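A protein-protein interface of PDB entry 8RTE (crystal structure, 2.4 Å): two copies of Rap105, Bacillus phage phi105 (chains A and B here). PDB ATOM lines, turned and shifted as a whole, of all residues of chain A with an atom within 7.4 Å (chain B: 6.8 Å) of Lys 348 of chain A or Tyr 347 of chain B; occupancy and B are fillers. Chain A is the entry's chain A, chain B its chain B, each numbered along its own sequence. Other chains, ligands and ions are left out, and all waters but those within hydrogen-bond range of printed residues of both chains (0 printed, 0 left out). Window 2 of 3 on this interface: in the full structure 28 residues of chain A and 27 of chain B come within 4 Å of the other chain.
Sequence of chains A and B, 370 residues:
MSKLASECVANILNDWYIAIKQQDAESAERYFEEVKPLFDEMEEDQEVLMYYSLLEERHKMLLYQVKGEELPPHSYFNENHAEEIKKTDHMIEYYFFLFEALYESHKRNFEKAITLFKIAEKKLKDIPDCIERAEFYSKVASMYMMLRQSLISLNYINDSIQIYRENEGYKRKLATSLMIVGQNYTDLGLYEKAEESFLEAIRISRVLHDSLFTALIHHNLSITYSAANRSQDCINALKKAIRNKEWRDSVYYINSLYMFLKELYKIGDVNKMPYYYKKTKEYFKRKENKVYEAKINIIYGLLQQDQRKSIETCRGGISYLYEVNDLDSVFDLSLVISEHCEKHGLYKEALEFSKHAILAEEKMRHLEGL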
ATOM      1  N   ARG A 315     -17.490 -25.039  10.891  1.00  0.00           N
ATOM      2  CA  ARG A 315     -16.801 -24.515   9.715  1.00  0.00           C
ATOM      3  C   ARG A 315     -16.985 -25.428   8.510  1.00  0.00           C
ATOM      4  O   ARG A 315     -17.188 -24.951   7.388  1.00  0.00           O
ATOM      5  CB  ARG A 315     -15.315 -24.348  10.014  1.00  0.00           C
ATOM      6  CG  ARG A 315     -14.973 -23.123  10.824  1.00  0.00           C
ATOM      7  CD  ARG A 315     -13.539 -23.204  11.281  1.00  0.00           C
ATOM      8  NE  ARG A 315     -13.154 -22.083  12.125  1.00  0.00           N
ATOM      9  CZ  ARG A 315     -12.155 -22.120  12.992  1.00  0.00           C
ATOM     10  NH1 ARG A 315     -11.415 -23.205  13.144  1.00  0.00           N
ATOM     11  NH2 ARG A 315     -11.884 -21.037  13.717  1.00  0.00           N
ATOM     12  N   CYS A 341     -21.713 -19.380  20.363  1.00  0.00           N
ATOM     13  CA  CYS A 341     -20.407 -18.929  20.829  1.00  0.00           C
ATOM     14  C   CYS A 341     -20.541 -17.746  21.781  1.00  0.00           C
ATOM     15  O   CYS A 341     -19.829 -17.671  22.792  1.00  0.00           O
ATOM     16  CB  CYS A 341     -19.534 -18.568  19.632  1.00  0.00           C
ATOM     17  SG  CYS A 341     -19.253 -19.955  18.518  1.00  0.00           S
ATOM     18  N   GLY A 345     -18.998 -17.205  25.697  1.00  0.00           N
ATOM     19  CA  GLY A 345     -17.891 -16.273  25.826  1.00  0.00           C
ATOM     20  C   GLY A 345     -16.825 -16.370  24.761  1.00  0.00           C
ATOM     21  O   GLY A 345     -15.775 -15.734  24.901  1.00  0.00           O
ATOM     22  N   LEU A 346     -17.057 -17.139  23.695  1.00  0.00           N
ATOM     23  CA  LEU A 346     -16.080 -17.285  22.616  1.00  0.00           C
ATOM     24  C   LEU A 346     -16.378 -16.209  21.574  1.00  0.00           C
ATOM     25  O   LEU A 346     -16.931 -16.460  20.499  1.00  0.00           O
ATOM     26  CB  LEU A 346     -16.126 -18.690  22.025  1.00  0.00           C
ATOM     27  CG  LEU A 346     -16.112 -19.820  23.058  1.00  0.00           C
ATOM     28  CD1 LEU A 346     -16.308 -21.170  22.383  1.00  0.00           C
ATOM     29  CD2 LEU A 346     -14.836 -19.803  23.900  1.00  0.00           C
ATOM     30  N   TYR A 347     -15.993 -14.978  21.915  1.00  0.00           N
ATOM     31  CA  TYR A 347     -16.387 -13.829  21.108  1.00  0.00           C
ATOM     32  C   TYR A 347     -15.666 -13.794  19.768  1.00  0.00           C
ATOM     33  O   TYR A 347     -16.236 -13.313  18.781  1.00  0.00           O
ATOM     34  CB  TYR A 347     -16.160 -12.545  21.899  1.00  0.00           C
ATOM     35  CG  TYR A 347     -17.009 -12.471  23.146  1.00  0.00           C
ATOM     36  CD1 TYR A 347     -18.391 -12.339  23.058  1.00  0.00           C
ATOM     37  CD2 TYR A 347     -16.438 -12.546  24.408  1.00  0.00           C
ATOM     38  CE1 TYR A 347     -19.177 -12.278  24.191  1.00  0.00           C
ATOM     39  CE2 TYR A 347     -17.216 -12.484  25.549  1.00  0.00           C
ATOM     40  CZ  TYR A 347     -18.584 -12.350  25.436  1.00  0.00           C
ATOM     41  OH  TYR A 347     -19.356 -12.287  26.573  1.00  0.00           O
ATOM     42  N   LYS A 348     -14.421 -14.275  19.706  1.00  0.00           N
ATOM     43  CA  LYS A 348     -13.728 -14.322  18.424  1.00  0.00           C
ATOM     44  C   LYS A 348     -14.477 -15.204  17.432  1.00  0.00           C
ATOM     45  O   LYS A 348     -14.635 -14.844  16.262  1.00  0.00           O
ATOM     46  CB  LYS A 348     -12.293 -14.818  18.604  1.00  0.00           C
ATOM     47  CG  LYS A 348     -11.462 -14.662  17.332  1.00  0.00           C
ATOM     48  CD  LYS A 348      -9.991 -14.997  17.541  1.00  0.00           C
ATOM     49  CE  LYS A 348      -9.334 -15.318  16.203  1.00  0.00           C
ATOM     50  NZ  LYS A 348      -8.131 -16.190  16.324  1.00  0.00           N
ATOM     51  N   GLU A 349     -14.951 -16.363  17.884  1.00  0.00           N
ATOM     52  CA  GLU A 349     -15.690 -17.265  17.008  1.00  0.00           C
ATOM     53  C   GLU A 349     -17.112 -16.778  16.760  1.00  0.00           C
ATOM     54  O   GLU A 349     -17.661 -16.991  15.671  1.00  0.00           O
ATOM     55  CB  GLU A 349     -15.693 -18.684  17.586  1.00  0.00           C
ATOM     56  CG  GLU A 349     -14.314 -19.305  17.679  1.00  0.00           C
ATOM     57  CD  GLU A 349     -13.494 -18.815  18.866  1.00  0.00           C
ATOM     58  OE1 GLU A 349     -13.934 -17.890  19.586  1.00  0.00           O
ATOM     59  OE2 GLU A 349     -12.382 -19.353  19.065  1.00  0.00           O
ATOM     60  N   ALA A 350     -17.735 -16.151  17.765  1.00  0.00           N
ATOM     61  CA  ALA A 350     -19.052 -15.556  17.548  1.00  0.00           C
ATOM     62  C   ALA A 350     -18.998 -14.524  16.434  1.00  0.00           C
ATOM     63  O   ALA A 350     -19.911 -14.443  15.602  1.00  0.00           O
ATOM     64  CB  ALA A 350     -19.574 -14.921  18.834  1.00  0.00           C
ATOM     65  N   LEU A 351     -17.943 -13.709  16.427  1.00  0.00           N
ATOM     66  CA  LEU A 351     -17.746 -12.744  15.356  1.00  0.00           C
ATOM     67  C   LEU A 351     -17.471 -13.442  14.029  1.00  0.00           C
ATOM     68  O   LEU A 351     -17.972 -13.012  12.983  1.00  0.00           O
ATOM     69  CB  LEU A 351     -16.603 -11.796  15.726  1.00  0.00           C
ATOM     70  CG  LEU A 351     -16.097 -10.890  14.600  1.00  0.00           C
ATOM     71  CD1 LEU A 351     -17.099  -9.793  14.299  1.00  0.00           C
ATOM     72  CD2 LEU A 351     -14.733 -10.309  14.933  1.00  0.00           C
ATOM     73  N   GLU A 352     -16.697 -14.534  14.057  1.00  0.00           N
ATOM     74  CA  GLU A 352     -16.362 -15.241  12.823  1.00  0.00           C
ATOM     75  C   GLU A 352     -17.615 -15.691  12.079  1.00  0.00           C
ATOM     76  O   GLU A 352     -17.677 -15.609  10.845  1.00  0.00           O
ATOM     77  CB  GLU A 352     -15.462 -16.438  13.130  1.00  0.00           C
ATOM     78  CG  GLU A 352     -15.334 -17.426  11.966  1.00  0.00           C
ATOM     79  CD  GLU A 352     -14.591 -18.695  12.340  1.00  0.00           C
ATOM     80  OE1 GLU A 352     -14.100 -18.783  13.486  1.00  0.00           O
ATOM     81  OE2 GLU A 352     -14.479 -19.600  11.484  1.00  0.00           O
ATOM     82  N   PHE A 353     -18.621 -16.175  12.808  1.00  0.00           N
ATOM     83  CA  PHE A 353     -19.861 -16.607  12.181  1.00  0.00           C
ATOM     84  C   PHE A 353     -20.888 -15.489  12.062  1.00  0.00           C
ATOM     85  O   PHE A 353     -21.770 -15.569  11.198  1.00  0.00           O
ATOM     86  CB  PHE A 353     -20.435 -17.797  12.943  1.00  0.00           C
ATOM     87  CG  PHE A 353     -19.621 -19.039  12.778  1.00  0.00           C
ATOM     88  CD1 PHE A 353     -19.827 -19.886  11.703  1.00  0.00           C
ATOM     89  CD2 PHE A 353     -18.614 -19.346  13.685  1.00  0.00           C
ATOM     90  CE1 PHE A 353     -19.057 -21.028  11.547  1.00  0.00           C
ATOM     91  CE2 PHE A 353     -17.847 -20.477  13.535  1.00  0.00           C
ATOM     92  CZ  PHE A 353     -18.069 -21.323  12.463  1.00  0.00           C
ATOM     93  N   SER A 354     -20.796 -14.461  12.911  1.00  0.00           N
ATOM     94  CA  SER A 354     -21.506 -13.214  12.647  1.00  0.00           C
ATOM     95  C   SER A 354     -21.137 -12.651  11.284  1.00  0.00           C
ATOM     96  O   SER A 354     -22.000 -12.127  10.568  1.00  0.00           O
ATOM     97  CB  SER A 354     -21.204 -12.191  13.741  1.00  0.00           C
ATOM     98  OG  SER A 354     -22.114 -11.114  13.682  1.00  0.00           O
ATOM     99  N   LYS A 355     -19.852 -12.736  10.915  1.00  0.00           N
ATOM    100  CA  LYS A 355     -19.411 -12.227   9.619  1.00  0.00           C
ATOM    101  C   LYS A 355     -19.940 -13.095   8.485  1.00  0.00           C
ATOM    102  O   LYS A 355     -20.333 -12.581   7.429  1.00  0.00           O
ATOM    103  CB  LYS A 355     -17.882 -12.156   9.568  1.00  0.00           C
ATOM    104  CG  LYS A 355     -17.252 -11.131  10.510  1.00  0.00           C
ATOM    105  CD  LYS A 355     -15.724 -11.207  10.499  1.00  0.00           C
ATOM    106  N   SER B 338     -16.820  -2.742  13.645  1.00  0.00           N
ATOM    107  CA  SER B 338     -16.545  -4.151  13.908  1.00  0.00           C
ATOM    108  C   SER B 338     -15.169  -4.550  13.381  1.00  0.00           C
ATOM    109  O   SER B 338     -14.384  -5.191  14.089  1.00  0.00           O
ATOM    110  CB  SER B 338     -17.646  -5.013  13.290  1.00  0.00           C
ATOM    111  OG  SER B 338     -17.413  -6.394  13.517  1.00  0.00           O
ATOM    112  N   CYS B 341     -12.529  -3.005  15.734  1.00  0.00           N
ATOM    113  CA  CYS B 341     -12.372  -3.768  16.971  1.00  0.00           C
ATOM    114  C   CYS B 341     -11.717  -5.126  16.721  1.00  0.00           C
ATOM    115  O   CYS B 341     -10.860  -5.557  17.503  1.00  0.00           O
ATOM    116  CB  CYS B 341     -13.727  -3.942  17.659  1.00  0.00           C
ATOM    117  SG  CYS B 341     -14.547  -2.411  18.176  1.00  0.00           S
ATOM    118  N   GLU B 342     -12.120  -5.825  15.653  1.00  0.00           N
ATOM    119  CA  GLU B 342     -11.517  -7.121  15.332  1.00  0.00           C
ATOM    120  C   GLU B 342     -10.003  -7.013  15.211  1.00  0.00           C
ATOM    121  O   GLU B 342      -9.258  -7.834  15.758  1.00  0.00           O
ATOM    122  CB  GLU B 342     -12.106  -7.673  14.033  1.00  0.00           C
ATOM    123  CG  GLU B 342     -11.647  -9.091  13.701  1.00  0.00           C
ATOM    124  CD  GLU B 342     -12.281  -9.642  12.435  1.00  0.00           C
ATOM    125  OE1 GLU B 342     -13.084  -8.922  11.807  1.00  0.00           O
ATOM    126  OE2 GLU B 342     -11.976 -10.798  12.070  1.00  0.00           O
ATOM    127  N   LYS B 343      -9.534  -5.993  14.494  1.00  0.00           N
ATOM    128  CA  LYS B 343      -8.110  -5.802  14.247  1.00  0.00           C
ATOM    129  C   LYS B 343      -7.341  -5.473  15.517  1.00  0.00           C
ATOM    130  O   LYS B 343      -6.130  -5.720  15.578  1.00  0.00           O
ATOM    131  CB  LYS B 343      -7.937  -4.689  13.216  1.00  0.00           C
ATOM    132  CG  LYS B 343      -8.185  -5.169  11.810  1.00  0.00           C
ATOM    133  CD  LYS B 343      -8.418  -4.055  10.806  1.00  0.00           C
ATOM    134  CE  LYS B 343      -7.638  -4.288   9.532  1.00  0.00           C
ATOM    135  NZ  LYS B 343      -8.086  -3.336   8.470  1.00  0.00           N
ATOM    136  N   HIS B 344      -8.014  -4.933  16.530  1.00  0.00           N
ATOM    137  CA  HIS B 344      -7.398  -4.595  17.805  1.00  0.00           C
ATOM    138  C   HIS B 344      -7.651  -5.643  18.879  1.00  0.00           C
ATOM    139  O   HIS B 344      -7.406  -5.373  20.058  1.00  0.00           O
ATOM    140  CB  HIS B 344      -7.882  -3.222  18.274  1.00  0.00           C
ATOM    141  CG  HIS B 344      -7.366  -2.091  17.439  1.00  0.00           C
ATOM    142  ND1 HIS B 344      -6.480  -1.154  17.926  1.00  0.00           N
ATOM    143  CD2 HIS B 344      -7.593  -1.756  16.147  1.00  0.00           C
ATOM    144  CE1 HIS B 344      -6.192  -0.286  16.974  1.00  0.00           C
ATOM    145  NE2 HIS B 344      -6.854  -0.628  15.883  1.00  0.00           N
ATOM    146  N   GLY B 345      -8.138  -6.827  18.503  1.00  0.00           N
ATOM    147  CA  GLY B 345      -8.386  -7.898  19.451  1.00  0.00           C
ATOM    148  C   GLY B 345      -9.585  -7.719  20.355  1.00  0.00           C
ATOM    149  O   GLY B 345      -9.752  -8.501  21.296  1.00  0.00           O
ATOM    150  N   LEU B 346     -10.430  -6.722  20.100  1.00  0.00           N
ATOM    151  CA  LEU B 346     -11.637  -6.486  20.900  1.00  0.00           C
ATOM    152  C   LEU B 346     -12.826  -7.209  20.261  1.00  0.00           C
ATOM    153  O   LEU B 346     -13.703  -6.610  19.634  1.00  0.00           O
ATOM    154  CB  LEU B 346     -11.895  -4.989  21.034  1.00  0.00           C
ATOM    155  CG  LEU B 346     -10.700  -4.121  21.434  1.00  0.00           C
ATOM    156  CD1 LEU B 346     -11.056  -2.646  21.347  1.00  0.00           C
ATOM    157  CD2 LEU B 346     -10.242  -4.470  22.842  1.00  0.00           C
ATOM    158  N   TYR B 347     -12.847  -8.536  20.441  1.00  0.00           N
ATOM    159  CA  TYR B 347     -13.813  -9.363  19.719  1.00  0.00           C
ATOM    160  C   TYR B 347     -15.227  -9.195  20.261  1.00  0.00           C
ATOM    161  O   TYR B 347     -16.196  -9.220  19.493  1.00  0.00           O
ATOM    162  CB  TYR B 347     -13.390 -10.830  19.777  1.00  0.00           C
ATOM    163  CG  TYR B 347     -12.037 -11.074  19.160  1.00  0.00           C
ATOM    164  CD1 TYR B 347     -11.842 -10.917  17.797  1.00  0.00           C
ATOM    165  CD2 TYR B 347     -10.950 -11.445  19.943  1.00  0.00           C
ATOM    166  CE1 TYR B 347     -10.601 -11.125  17.224  1.00  0.00           C
ATOM    167  CE2 TYR B 347      -9.704 -11.659  19.382  1.00  0.00           C
ATOM    168  CZ  TYR B 347      -9.536 -11.497  18.019  1.00  0.00           C
ATOM    169  OH  TYR B 347      -8.302 -11.706  17.445  1.00  0.00           O
ATOM    170  N   LYS B 348     -15.368  -9.013  21.575  1.00  0.00           N
ATOM    171  CA  LYS B 348     -16.691  -8.798  22.154  1.00  0.00           C
ATOM    172  C   LYS B 348     -17.342  -7.547  21.576  1.00  0.00           C
ATOM    173  O   LYS B 348     -18.531  -7.551  21.241  1.00  0.00           O
ATOM    174  CB  LYS B 348     -16.591  -8.692  23.676  1.00  0.00           C
ATOM    175  CG  LYS B 348     -17.938  -8.670  24.386  1.00  0.00           C
ATOM    176  CD  LYS B 348     -17.764  -8.712  25.897  1.00  0.00           C
ATOM    177  CE  LYS B 348     -18.994  -8.168  26.609  1.00  0.00           C
ATOM    178  NZ  LYS B 348     -18.633  -7.634  27.958  1.00  0.00           N
ATOM    179  N   GLU B 349     -16.568  -6.471  21.446  1.00  0.00           N
ATOM    180  CA  GLU B 349     -17.093  -5.227  20.898  1.00  0.00           C
ATOM    181  C   GLU B 349     -17.264  -5.331  19.387  1.00  0.00           C
ATOM    182  O   GLU B 349     -18.209  -4.771  18.821  1.00  0.00           O
ATOM    183  CB  GLU B 349     -16.161  -4.066  21.259  1.00  0.00           C
ATOM    184  CG  GLU B 349     -15.976  -3.825  22.762  1.00  0.00           C
ATOM    185  CD  GLU B 349     -15.012  -4.820  23.410  1.00  0.00           C
ATOM    186  OE1 GLU B 349     -14.584  -5.774  22.725  1.00  0.00           O
ATOM    187  OE2 GLU B 349     -14.689  -4.659  24.605  1.00  0.00           O
ATOM    188  N   ALA B 350     -16.351  -6.043  18.720  1.00  0.00           N
ATOM    189  CA  ALA B 350     -16.500  -6.301  17.292  1.00  0.00           C
ATOM    190  C   ALA B 350     -17.789  -7.055  16.999  1.00  0.00           C
ATOM    191  O   ALA B 350     -18.520  -6.705  16.066  1.00  0.00           O
ATOM    192  CB  ALA B 350     -15.296  -7.081  16.775  1.00  0.00           C
ATOM    193  N   LEU B 351     -18.097  -8.078  17.802  1.00  0.00           N
ATOM    194  CA  LEU B 351     -19.346  -8.807  17.616  1.00  0.00           C
ATOM    195  C   LEU B 351     -20.551  -7.919  17.901  1.00  0.00           C
ATOM    196  O   LEU B 351     -21.560  -7.990  17.192  1.00  0.00           O
ATOM    197  CB  LEU B 351     -19.372 -10.045  18.513  1.00  0.00           C
ATOM    198  CG  LEU B 351     -20.707 -10.788  18.624  1.00  0.00           C
ATOM    199  CD1 LEU B 351     -21.021 -11.571  17.359  1.00  0.00           C
ATOM    200  CD2 LEU B 351     -20.729 -11.685  19.847  1.00  0.00           C
ATOM    201  N   GLU B 352     -20.452  -7.063  18.924  1.00  0.00           N
ATOM    202  CA  GLU B 352     -21.562  -6.186  19.281  1.00  0.00           C
ATOM    203  C   GLU B 352     -21.976  -5.303  18.108  1.00  0.00           C
ATOM    204  O   GLU B 352     -23.172  -5.123  17.848  1.00  0.00           O
ATOM    205  CB  GLU B 352     -21.169  -5.334  20.486  1.00  0.00           C
ATOM    206  CG  GLU B 352     -22.092  -4.152  20.757  1.00  0.00           C
ATOM    207  CD  GLU B 352     -21.511  -3.201  21.787  1.00  0.00           C
ATOM    208  OE1 GLU B 352     -20.436  -3.513  22.344  1.00  0.00           O
ATOM    209  OE2 GLU B 352     -22.111  -2.130  22.019  1.00  0.00           O
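Among the printed residues, pairs that only touch across the chains: Leu 351 of chain A with Ser 338 of chain B (3.5 Å), Leu 351 of chain A with Glu 342 of chain B (3.5 Å), Ala 350 of chain A with Leu 351 of chain B (3.5 Å), Lys 348 of chain A with Tyr 347 of chain B (3.6 Å), Tyr 347 of chain A with Lys 348 of chain B (3.6 Å), Ser 354 of chain A with Leu 351 of chain B (3.7 Å), Lys 355 of chain A with Glu 342 of chain B (3.7 Å), Tyr 347 of chain A with Tyr 347 of chain B (3.7 Å), Leu 351 of chain A with Ala 350 of chain B (3.8 Å) and Leu 351 of chain A with Leu 351 of chain B (3.9 Å).
Tyr 347 of chain B touches its own counterpart, Tyr 347 of chain A.
Tyr 347 of chain A touches Lys 348 of chain B, and with the chains exchanged Lys 348 of chain A touches Tyr 347 of chain B.
Ala 350 of chain A touches Leu 351 of chain B, and with the chains exchanged Leu 351 of chain A touches Ala 350 of chain B.
Leu 351 of chain B touches its own counterpart, Leu 351 of chain A.
Of the 10 pairs that touch across the chains among the printed residues, 6 have their exchanged pair printed and touching as well.
Of the 13 printed residues of chain B, 6 touch a printed residue of chain A.
Hydrophobic or aromatic side chains of chain B within 4 Å of the printed part of chain A: Tyr 347, Ala 350 and Leu 351.
Along chain B the printed residues that touch a printed residue of chain A span positions 338 to 351.
Of the 13 printed residues of chain A, 6 touch a printed residue of chain B.
Among the printed residues, no Asp or Glu carboxylate lies within 4 Å of a Lys or Arg side-chain nitrogen of the other chain.
Lys 348 of chain A touches just one residue of chain B: Tyr 347.
Of the printed residues of chain B, Lys 355 of chain A touches Glu 342 (3.7 Å).
Printed residues of chain A within 4 Å of Glu 342 of chain B: Leu 351 (3.5 Å) and Lys 355 (3.7 Å).
Tyr 347 of chain B touches two residues of chain A.
Of the printed residues of chain A, Lys 348 of chain B touches Tyr 347 (3.6 Å).
The side-chain hydroxyl (OG) of Ser 338 of chain B is in hydrogen-bond range of the backbone carbonyl oxygen (O) of Ala 350 of chain B, 2.8 Å away.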
